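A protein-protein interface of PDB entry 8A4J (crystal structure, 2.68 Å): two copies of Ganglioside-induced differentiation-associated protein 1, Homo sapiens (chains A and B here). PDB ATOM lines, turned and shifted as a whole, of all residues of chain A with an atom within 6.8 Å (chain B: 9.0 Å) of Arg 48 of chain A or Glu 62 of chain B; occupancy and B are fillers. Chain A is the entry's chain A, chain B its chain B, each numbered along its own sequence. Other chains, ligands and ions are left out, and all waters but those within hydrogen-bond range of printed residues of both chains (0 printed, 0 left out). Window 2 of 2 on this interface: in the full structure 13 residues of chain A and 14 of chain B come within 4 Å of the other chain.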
ATOM      1  N   HIS A   8     -31.931   1.788  11.876  1.00  0.00           N
ATOM      2  CA  HIS A   8     -32.677   2.685  11.010  1.00  0.00           C
ATOM      3  C   HIS A   8     -32.500   4.109  11.502  1.00  0.00           C
ATOM      4  O   HIS A   8     -32.070   4.340  12.649  1.00  0.00           O
ATOM      5  CB  HIS A   8     -34.160   2.351  11.053  1.00  0.00           C
ATOM      6  CG  HIS A   8     -34.771   2.670  12.385  1.00  0.00           C
ATOM      7  ND1 HIS A   8     -35.649   3.711  12.582  1.00  0.00           N
ATOM      8  CD2 HIS A   8     -34.556   2.125  13.609  1.00  0.00           C
ATOM      9  CE1 HIS A   8     -35.993   3.755  13.859  1.00  0.00           C
ATOM     10  NE2 HIS A   8     -35.352   2.792  14.502  1.00  0.00           N
ATOM     11  N   TRP A   9     -32.905   5.061  10.630  1.00  0.00           N
ATOM     12  CA  TRP A   9     -33.162   6.439  11.041  1.00  0.00           C
ATOM     13  C   TRP A   9     -34.650   6.706  11.117  1.00  0.00           C
ATOM     14  O   TRP A   9     -35.336   6.776  10.084  1.00  0.00           O
ATOM     15  CB  TRP A   9     -32.602   7.467  10.085  1.00  0.00           C
ATOM     16  CG  TRP A   9     -31.260   7.290   9.761  1.00  0.00           C
ATOM     17  CD1 TRP A   9     -30.197   7.942  10.283  1.00  0.00           C
ATOM     18  CD2 TRP A   9     -30.767   6.339   8.840  1.00  0.00           C
ATOM     19  NE1 TRP A   9     -29.041   7.469   9.699  1.00  0.00           N
ATOM     20  CE2 TRP A   9     -29.373   6.484   8.801  1.00  0.00           C
ATOM     21  CE3 TRP A   9     -31.379   5.361   8.029  1.00  0.00           C
ATOM     22  CZ2 TRP A   9     -28.559   5.685   7.976  1.00  0.00           C
ATOM     23  CZ3 TRP A   9     -30.560   4.566   7.198  1.00  0.00           C
ATOM     24  CH2 TRP A   9     -29.174   4.728   7.189  1.00  0.00           C
ATOM     25  N   VAL A  34     -30.514   4.995  14.907  1.00  0.00           N
ATOM     26  CA  VAL A  34     -29.094   5.343  14.989  1.00  0.00           C
ATOM     27  C   VAL A  34     -28.861   6.842  14.957  1.00  0.00           C
ATOM     28  O   VAL A  34     -27.739   7.295  15.256  1.00  0.00           O
ATOM     29  CB  VAL A  34     -28.256   4.820  13.815  1.00  0.00           C
ATOM     30  CG1 VAL A  34     -28.407   3.408  13.697  1.00  0.00           C
ATOM     31  CG2 VAL A  34     -28.700   5.477  12.494  1.00  0.00           C
ATOM     32  N   SER A  35     -29.884   7.614  14.590  1.00  0.00           N
ATOM     33  CA  SER A  35     -29.746   9.040  14.361  1.00  0.00           C
ATOM     34  C   SER A  35     -29.503   9.757  15.679  1.00  0.00           C
ATOM     35  O   SER A  35     -29.807   9.241  16.768  1.00  0.00           O
ATOM     36  CB  SER A  35     -30.998   9.590  13.702  1.00  0.00           C
ATOM     37  OG  SER A  35     -32.057   9.373  14.584  1.00  0.00           O
ATOM     38  N   LEU A  36     -28.945  10.996  15.556  1.00  0.00           N
ATOM     39  CA  LEU A  36     -28.613  11.864  16.672  1.00  0.00           C
ATOM     40  C   LEU A  36     -29.439  13.137  16.685  1.00  0.00           C
ATOM     41  O   LEU A  36     -29.754  13.705  15.629  1.00  0.00           O
ATOM     42  CB  LEU A  36     -27.145  12.269  16.628  1.00  0.00           C
ATOM     43  CG  LEU A  36     -26.185  11.147  17.001  1.00  0.00           C
ATOM     44  CD1 LEU A  36     -24.798  11.538  16.549  1.00  0.00           C
ATOM     45  CD2 LEU A  36     -26.288  10.897  18.491  1.00  0.00           C
ATOM     46  N   PRO A  37     -29.772  13.639  17.872  1.00  0.00           N
ATOM     47  CA  PRO A  37     -30.550  14.892  17.913  1.00  0.00           C
ATOM     48  C   PRO A  37     -29.821  16.016  17.192  1.00  0.00           C
ATOM     49  O   PRO A  37     -30.397  16.688  16.324  1.00  0.00           O
ATOM     50  CB  PRO A  37     -30.710  15.160  19.421  1.00  0.00           C
ATOM     51  CG  PRO A  37     -30.455  13.839  20.098  1.00  0.00           C
ATOM     52  CD  PRO A  37     -29.469  13.103  19.212  1.00  0.00           C
ATOM     53  N   LEU A  38     -28.552  16.230  17.532  1.00  0.00           N
ATOM     54  CA  LEU A  38     -27.720  17.260  16.934  1.00  0.00           C
ATOM     55  C   LEU A  38     -26.542  16.624  16.203  1.00  0.00           C
ATOM     56  O   LEU A  38     -25.914  15.685  16.704  1.00  0.00           O
ATOM     57  CB  LEU A  38     -27.218  18.228  18.010  1.00  0.00           C
ATOM     58  CG  LEU A  38     -28.267  19.093  18.718  1.00  0.00           C
ATOM     59  CD1 LEU A  38     -27.674  19.887  19.869  1.00  0.00           C
ATOM     60  CD2 LEU A  38     -28.892  20.031  17.704  1.00  0.00           C
ATOM     61  N   SER A  39     -26.240  17.154  15.024  1.00  0.00           N
ATOM     62  CA  SER A  39     -25.114  16.679  14.250  1.00  0.00           C
ATOM     63  C   SER A  39     -23.829  17.367  14.702  1.00  0.00           C
ATOM     64  O   SER A  39     -23.830  18.247  15.569  1.00  0.00           O
ATOM     65  CB  SER A  39     -25.339  16.935  12.765  1.00  0.00           C
ATOM     66  OG  SER A  39     -25.472  18.315  12.507  1.00  0.00           O
ATOM     67  N   GLU A  40     -22.713  16.960  14.084  1.00  0.00           N
ATOM     68  CA  GLU A  40     -21.424  17.565  14.402  1.00  0.00           C
ATOM     69  C   GLU A  40     -21.444  19.066  14.149  1.00  0.00           C
ATOM     70  O   GLU A  40     -20.780  19.822  14.864  1.00  0.00           O
ATOM     71  CB  GLU A  40     -20.312  16.903  13.575  1.00  0.00           C
ATOM     72  CG  GLU A  40     -20.053  15.434  13.944  1.00  0.00           C
ATOM     73  CD  GLU A  40     -19.126  14.732  12.972  1.00  0.00           C
ATOM     74  OE1 GLU A  40     -18.217  15.399  12.437  1.00  0.00           O
ATOM     75  OE2 GLU A  40     -19.310  13.515  12.743  1.00  0.00           O
ATOM     76  N   GLU A  43     -26.982  20.492  13.984  1.00  0.00           N
ATOM     77  CA  GLU A  43     -28.131  20.609  13.111  1.00  0.00           C
ATOM     78  C   GLU A  43     -29.123  19.519  13.500  1.00  0.00           C
ATOM     79  O   GLU A  43     -28.716  18.396  13.826  1.00  0.00           O
ATOM     80  CB  GLU A  43     -27.742  20.464  11.629  1.00  0.00           C
ATOM     81  CG  GLU A  43     -26.834  21.561  11.090  1.00  0.00           C
ATOM     82  CD  GLU A  43     -26.621  21.489   9.582  1.00  0.00           C
ATOM     83  OE1 GLU A  43     -26.417  20.383   9.060  1.00  0.00           O
ATOM     84  OE2 GLU A  43     -26.652  22.548   8.917  1.00  0.00           O
ATOM     85  N   PRO A  44     -30.414  19.839  13.529  1.00  0.00           N
ATOM     86  CA  PRO A  44     -31.453  18.865  13.873  1.00  0.00           C
ATOM     87  C   PRO A  44     -31.930  18.033  12.682  1.00  0.00           C
ATOM     88  O   PRO A  44     -31.599  18.302  11.531  1.00  0.00           O
ATOM     89  CB  PRO A  44     -32.579  19.764  14.400  1.00  0.00           C
ATOM     90  CG  PRO A  44     -32.387  21.060  13.662  1.00  0.00           C
ATOM     91  CD  PRO A  44     -30.930  21.225  13.489  1.00  0.00           C
ATOM     92  N   TRP A  45     -32.767  17.020  12.986  1.00  0.00           N
ATOM     93  CA  TRP A  45     -33.141  16.038  11.961  1.00  0.00           C
ATOM     94  C   TRP A  45     -33.709  16.727  10.705  1.00  0.00           C
ATOM     95  O   TRP A  45     -33.463  16.264   9.590  1.00  0.00           O
ATOM     96  CB  TRP A  45     -34.127  14.939  12.552  1.00  0.00           C
ATOM     97  CG  TRP A  45     -35.561  15.451  12.829  1.00  0.00           C
ATOM     98  CD1 TRP A  45     -36.055  15.911  14.028  1.00  0.00           C
ATOM     99  CD2 TRP A  45     -36.634  15.577  11.886  1.00  0.00           C
ATOM    100  NE1 TRP A  45     -37.348  16.405  13.862  1.00  0.00           N
ATOM    101  CE2 TRP A  45     -37.735  16.177  12.569  1.00  0.00           C
ATOM    102  CE3 TRP A  45     -36.770  15.256  10.535  1.00  0.00           C
ATOM    103  CZ2 TRP A  45     -38.950  16.477  11.938  1.00  0.00           C
ATOM    104  CZ3 TRP A  45     -37.957  15.581   9.894  1.00  0.00           C
ATOM    105  CH2 TRP A  45     -39.052  16.178  10.609  1.00  0.00           C
ATOM    106  N   PHE A  46     -34.435  17.844  10.846  1.00  0.00           N
ATOM    107  CA  PHE A  46     -35.015  18.494   9.661  1.00  0.00           C
ATOM    108  C   PHE A  46     -33.981  19.260   8.837  1.00  0.00           C
ATOM    109  O   PHE A  46     -34.369  19.932   7.876  1.00  0.00           O
ATOM    110  CB  PHE A  46     -36.215  19.458   9.978  1.00  0.00           C
ATOM    111  CG  PHE A  46     -36.006  20.414  11.144  1.00  0.00           C
ATOM    112  CD1 PHE A  46     -36.164  19.972  12.441  1.00  0.00           C
ATOM    113  CD2 PHE A  46     -35.723  21.740  10.950  1.00  0.00           C
ATOM    114  CE1 PHE A  46     -35.973  20.817  13.534  1.00  0.00           C
ATOM    115  CE2 PHE A  46     -35.540  22.605  12.054  1.00  0.00           C
ATOM    116  CZ  PHE A  46     -35.662  22.135  13.339  1.00  0.00           C
ATOM    117  N   MET A  47     -32.714  19.284   9.249  1.00  0.00           N
ATOM    118  CA  MET A  47     -31.681  19.911   8.431  1.00  0.00           C
ATOM    119  C   MET A  47     -30.993  18.925   7.505  1.00  0.00           C
ATOM    120  O   MET A  47     -30.351  19.348   6.536  1.00  0.00           O
ATOM    121  CB  MET A  47     -30.567  20.495   9.276  1.00  0.00           C
ATOM    122  CG  MET A  47     -30.957  21.501  10.278  1.00  0.00           C
ATOM    123  SD  MET A  47     -31.394  23.134   9.744  1.00  0.00           S
ATOM    124  CE  MET A  47     -31.594  23.798  11.391  1.00  0.00           C
ATOM    125  N   ARG A  48     -31.094  17.638   7.794  1.00  0.00           N
ATOM    126  CA  ARG A  48     -30.129  16.680   7.301  1.00  0.00           C
ATOM    127  C   ARG A  48     -30.798  15.631   6.458  1.00  0.00           C
ATOM    128  O   ARG A  48     -30.640  14.437   6.704  1.00  0.00           O
ATOM    129  CB  ARG A  48     -29.417  16.022   8.470  1.00  0.00           C
ATOM    130  CG  ARG A  48     -29.093  16.976   9.602  1.00  0.00           C
ATOM    131  CD  ARG A  48     -28.639  16.167  10.804  1.00  0.00           C
ATOM    132  NE  ARG A  48     -27.628  15.221  10.351  1.00  0.00           N
ATOM    133  CZ  ARG A  48     -27.199  14.178  11.042  1.00  0.00           C
ATOM    134  NH1 ARG A  48     -27.624  13.947  12.270  1.00  0.00           N
ATOM    135  NH2 ARG A  48     -26.333  13.339  10.479  1.00  0.00           N
ATOM    136  N   LEU A  49     -31.565  16.057   5.471  1.00  0.00           N
ATOM    137  CA  LEU A  49     -32.269  15.101   4.633  1.00  0.00           C
ATOM    138  C   LEU A  49     -31.385  14.745   3.437  1.00  0.00           C
ATOM    139  O   LEU A  49     -30.936  15.634   2.691  1.00  0.00           O
ATOM    140  CB  LEU A  49     -33.635  15.652   4.227  1.00  0.00           C
ATOM    141  CG  LEU A  49     -34.642  15.625   5.403  1.00  0.00           C
ATOM    142  CD1 LEU A  49     -34.822  17.082   5.886  1.00  0.00           C
ATOM    143  CD2 LEU A  49     -35.949  14.967   5.099  1.00  0.00           C
ATOM    144  N   ASN A  50     -31.112  13.439   3.304  1.00  0.00           N
ATOM    145  CA  ASN A  50     -30.291  12.825   2.258  1.00  0.00           C
ATOM    146  C   ASN A  50     -30.488  11.297   2.287  1.00  0.00           C
ATOM    147  O   ASN A  50     -30.375  10.619   1.262  1.00  0.00           O
ATOM    148  CB  ASN A  50     -28.816  13.178   2.436  1.00  0.00           C
ATOM    149  CG  ASN A  50     -28.375  13.132   3.878  1.00  0.00           C
ATOM    150  OD1 ASN A  50     -28.249  12.070   4.480  1.00  0.00           O
ATOM    151  ND2 ASN A  50     -28.094  14.300   4.427  1.00  0.00           N
ATOM    152  N   ILE A 119     -35.663  21.522  -0.669  1.00  0.00           N
ATOM    153  CA  ILE A 119     -34.657  22.327   0.009  1.00  0.00           C
ATOM    154  C   ILE A 119     -34.054  23.357  -0.951  1.00  0.00           C
ATOM    155  O   ILE A 119     -33.850  24.518  -0.596  1.00  0.00           O
ATOM    156  CB  ILE A 119     -33.580  21.429   0.618  1.00  0.00           C
ATOM    157  CG1 ILE A 119     -34.209  20.665   1.795  1.00  0.00           C
ATOM    158  CG2 ILE A 119     -32.377  22.315   0.988  1.00  0.00           C
ATOM    159  CD1 ILE A 119     -33.526  19.356   2.112  1.00  0.00           C
ATOM    160  N   VAL B   2     -18.130   6.262  20.602  1.00  0.00           N
ATOM    161  CA  VAL B   2     -18.950   5.767  19.492  1.00  0.00           C
ATOM    162  C   VAL B   2     -18.511   4.359  19.113  1.00  0.00           C
ATOM    163  O   VAL B   2     -17.362   4.153  18.703  1.00  0.00           O
ATOM    164  CB  VAL B   2     -18.845   6.702  18.276  1.00  0.00           C
ATOM    165  CG1 VAL B   2     -19.412   6.048  17.026  1.00  0.00           C
ATOM    166  CG2 VAL B   2     -19.538   8.025  18.526  1.00  0.00           C
ATOM    167  N   LYS B   3     -19.441   3.406  19.172  1.00  0.00           N
ATOM    168  CA  LYS B   3     -19.142   2.004  18.891  1.00  0.00           C
ATOM    169  C   LYS B   3     -19.121   1.750  17.389  1.00  0.00           C
ATOM    170  O   LYS B   3     -19.888   2.339  16.617  1.00  0.00           O
ATOM    171  CB  LYS B   3     -20.179   1.091  19.566  1.00  0.00           C
ATOM    172  CG  LYS B   3     -20.143   1.141  21.099  1.00  0.00           C
ATOM    173  CD  LYS B   3     -21.349   0.487  21.784  1.00  0.00           C
ATOM    174  CE  LYS B   3     -21.535  -0.975  21.369  1.00  0.00           C
ATOM    175  NZ  LYS B   3     -20.268  -1.761  21.503  1.00  0.00           N
ATOM    176  N   LEU B  58     -22.085  -2.763   8.500  1.00  0.00           N
ATOM    177  CA  LEU B  58     -21.370  -1.995   9.510  1.00  0.00           C
ATOM    178  C   LEU B  58     -22.226  -0.819  10.013  1.00  0.00           C
ATOM    179  O   LEU B  58     -22.786  -0.023   9.228  1.00  0.00           O
ATOM    180  CB  LEU B  58     -20.020  -1.483   8.985  1.00  0.00           C
ATOM    181  CG  LEU B  58     -19.221  -0.669  10.008  1.00  0.00           C
ATOM    182  CD1 LEU B  58     -18.455  -1.552  10.912  1.00  0.00           C
ATOM    183  CD2 LEU B  58     -18.312   0.372   9.377  1.00  0.00           C
ATOM    184  N   ILE B  59     -22.274  -0.689  11.328  1.00  0.00           N
ATOM    185  CA  ILE B  59     -22.984   0.372  11.990  1.00  0.00           C
ATOM    186  C   ILE B  59     -21.953   1.121  12.795  1.00  0.00           C
ATOM    187  O   ILE B  59     -21.305   0.540  13.665  1.00  0.00           O
ATOM    188  CB  ILE B  59     -24.117  -0.167  12.878  1.00  0.00           C
ATOM    189  CG1 ILE B  59     -25.144  -0.895  12.017  1.00  0.00           C
ATOM    190  CG2 ILE B  59     -24.809   0.967  13.602  1.00  0.00           C
ATOM    191  CD1 ILE B  59     -25.214  -2.333  12.260  1.00  0.00           C
ATOM    192  N   HIS B  60     -21.781   2.398  12.475  1.00  0.00           N
ATOM    193  CA  HIS B  60     -20.797   3.291  13.090  1.00  0.00           C
ATOM    194  C   HIS B  60     -21.513   4.616  13.347  1.00  0.00           C
ATOM    195  O   HIS B  60     -21.747   5.383  12.410  1.00  0.00           O
ATOM    196  CB  HIS B  60     -19.565   3.498  12.192  1.00  0.00           C
ATOM    197  CG  HIS B  60     -18.613   4.490  12.763  1.00  0.00           C
ATOM    198  ND1 HIS B  60     -18.055   5.503  12.019  1.00  0.00           N
ATOM    199  CD2 HIS B  60     -18.194   4.679  14.038  1.00  0.00           C
ATOM    200  CE1 HIS B  60     -17.329   6.275  12.809  1.00  0.00           C
ATOM    201  NE2 HIS B  60     -17.395   5.795  14.040  1.00  0.00           N
ATOM    202  N   GLY B  61     -21.890   4.848  14.602  1.00  0.00           N
ATOM    203  CA  GLY B  61     -22.669   6.007  14.960  1.00  0.00           C
ATOM    204  C   GLY B  61     -23.965   6.000  14.189  1.00  0.00           C
ATOM    205  O   GLY B  61     -24.815   5.125  14.398  1.00  0.00           O
ATOM    206  N   GLU B  62     -24.085   6.938  13.260  1.00  0.00           N
ATOM    207  CA  GLU B  62     -25.295   7.127  12.493  1.00  0.00           C
ATOM    208  C   GLU B  62     -25.244   6.472  11.139  1.00  0.00           C
ATOM    209  O   GLU B  62     -26.257   6.464  10.424  1.00  0.00           O
ATOM    210  CB  GLU B  62     -25.553   8.615  12.252  1.00  0.00           C
ATOM    211  CG  GLU B  62     -25.755   9.443  13.470  1.00  0.00           C
ATOM    212  CD  GLU B  62     -25.947  10.885  13.109  1.00  0.00           C
ATOM    213  OE1 GLU B  62     -24.998  11.478  12.521  1.00  0.00           O
ATOM    214  OE2 GLU B  62     -27.055  11.414  13.372  1.00  0.00           O
ATOM    215  N   ASN B  63     -24.115   5.892  10.775  1.00  0.00           N
ATOM    216  CA  ASN B  63     -23.933   5.385   9.424  1.00  0.00           C
ATOM    217  C   ASN B  63     -24.169   3.887   9.426  1.00  0.00           C
ATOM    218  O   ASN B  63     -23.725   3.179  10.333  1.00  0.00           O
ATOM    219  CB  ASN B  63     -22.531   5.674   8.879  1.00  0.00           C
ATOM    220  CG  ASN B  63     -22.239   7.165   8.759  1.00  0.00           C
ATOM    221  OD1 ASN B  63     -21.784   7.800   9.711  1.00  0.00           O
ATOM    222  ND2 ASN B  63     -22.515   7.728   7.591  1.00  0.00           N
ATOM    223  N   ILE B  64     -24.904   3.434   8.419  1.00  0.00           N
ATOM    224  CA  ILE B  64     -25.126   2.027   8.142  1.00  0.00           C
ATOM    225  C   ILE B  64     -24.538   1.736   6.773  1.00  0.00           C
ATOM    226  O   ILE B  64     -25.012   2.278   5.766  1.00  0.00           O
ATOM    227  CB  ILE B  64     -26.625   1.698   8.160  1.00  0.00           C
ATOM    228  CG1 ILE B  64     -27.169   1.817   9.580  1.00  0.00           C
ATOM    229  CG2 ILE B  64     -26.902   0.284   7.663  1.00  0.00           C
ATOM    230  CD1 ILE B  64     -28.623   2.311   9.633  1.00  0.00           C
ATOM    231  N   ILE B  65     -23.603   0.806   6.710  1.00  0.00           N
ATOM    232  CA  ILE B  65     -22.981   0.466   5.440  1.00  0.00           C
ATOM    233  C   ILE B  65     -23.072  -1.033   5.183  1.00  0.00           C
ATOM    234  O   ILE B  65     -22.859  -1.848   6.090  1.00  0.00           O
ATOM    235  CB  ILE B  65     -21.514   0.955   5.393  1.00  0.00           C
ATOM    236  CG1 ILE B  65     -21.409   2.436   5.817  1.00  0.00           C
ATOM    237  CG2 ILE B  65     -20.977   0.883   3.978  1.00  0.00           C
ATOM    238  CD1 ILE B  65     -21.145   2.629   7.313  1.00  0.00           C
ATOM    239  N   TYR B  74     -15.623   2.884   3.421  1.00  0.00           N
ATOM    240  CA  TYR B  74     -16.054   3.713   4.546  1.00  0.00           C
ATOM    241  C   TYR B  74     -14.968   3.736   5.623  1.00  0.00           C
ATOM    242  O   TYR B  74     -14.596   4.807   6.142  1.00  0.00           O
ATOM    243  CB  TYR B  74     -17.391   3.197   5.101  1.00  0.00           C
ATOM    244  CG  TYR B  74     -17.791   3.942   6.355  1.00  0.00           C
ATOM    245  CD1 TYR B  74     -18.451   5.183   6.299  1.00  0.00           C
ATOM    246  CD2 TYR B  74     -17.476   3.426   7.602  1.00  0.00           C
ATOM    247  CE1 TYR B  74     -18.794   5.859   7.459  1.00  0.00           C
ATOM    248  CE2 TYR B  74     -17.794   4.116   8.773  1.00  0.00           C
ATOM    249  CZ  TYR B  74     -18.440   5.324   8.686  1.00  0.00           C
ATOM    250  OH  TYR B  74     -18.755   6.017   9.827  1.00  0.00           O
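Of the printed residues of chain B, Leu 36 of chain A touches Glu 62.
Of the printed residues of chain B, Trp 9 of chain A touches Glu 62 and Ile 64.
Val 2 of chain B touches none of the printed residues of chain A.
The nearest residue of chain B that does not touch Arg 48 of chain A is Asn 63 of chain B (7.2 Å).
Among the printed residues, pairs that only touch across the chains: Val 34 of chain A with Glu 62 of chain B (3.4 Å), Trp 9 of chain A with Ile 64 of chain B (3.5 Å), Val 34 of chain A with Gly 61 of chain B (3.5 Å) and Ser 35 of chain A with Glu 62 of chain B (3.7 Å).
O of Arg 48 of chain A lies within hydrogen-bond range of ND2 of Asn 50 of chain A (3.4 Å).
The backbone carbonyl oxygen (O) of His 8 of chain A is in hydrogen-bond range of the backbone NH (N) of Val 34 of chain A (2.8 Å).
No position is printed for both chains.
Of the 7 pairs that touch across the chains among the printed residues, none has its exchanged pair printed and touching as well.
The side-chain carboxylate (OE2) of Glu 62 of chain B sits at hydrogen-bond distance from the backbone NH (N) of Leu 36 of chain A (2.9 Å).
The guanidinium group (NH1) of Arg 48 of chain A lies within salt-bridge range of the side-chain carboxylate (OE2) of Glu 62 of chain B, 2.8 Å away.
The indole nitrogen (NE1) of Trp 9 of chain A is in hydrogen-bond range of the backbone carbonyl oxygen (O) of Glu 62 of chain B, 3.0 Å away.
Hydrophobic or aromatic side chains of chain B within 4 Å of the printed part of chain A: Ile 64.
Along chain B the printed residues that touch a printed residue of chain A span positions 61 to 64.
Of the 18 printed residues of chain A, 5 touch a printed residue of chain B.
Among the printed residues, Asp or Glu carboxylates within 4 Å of a Lys or Arg side-chain nitrogen of the other chain: Arg 48 of chain A with Glu 62 of chain B.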
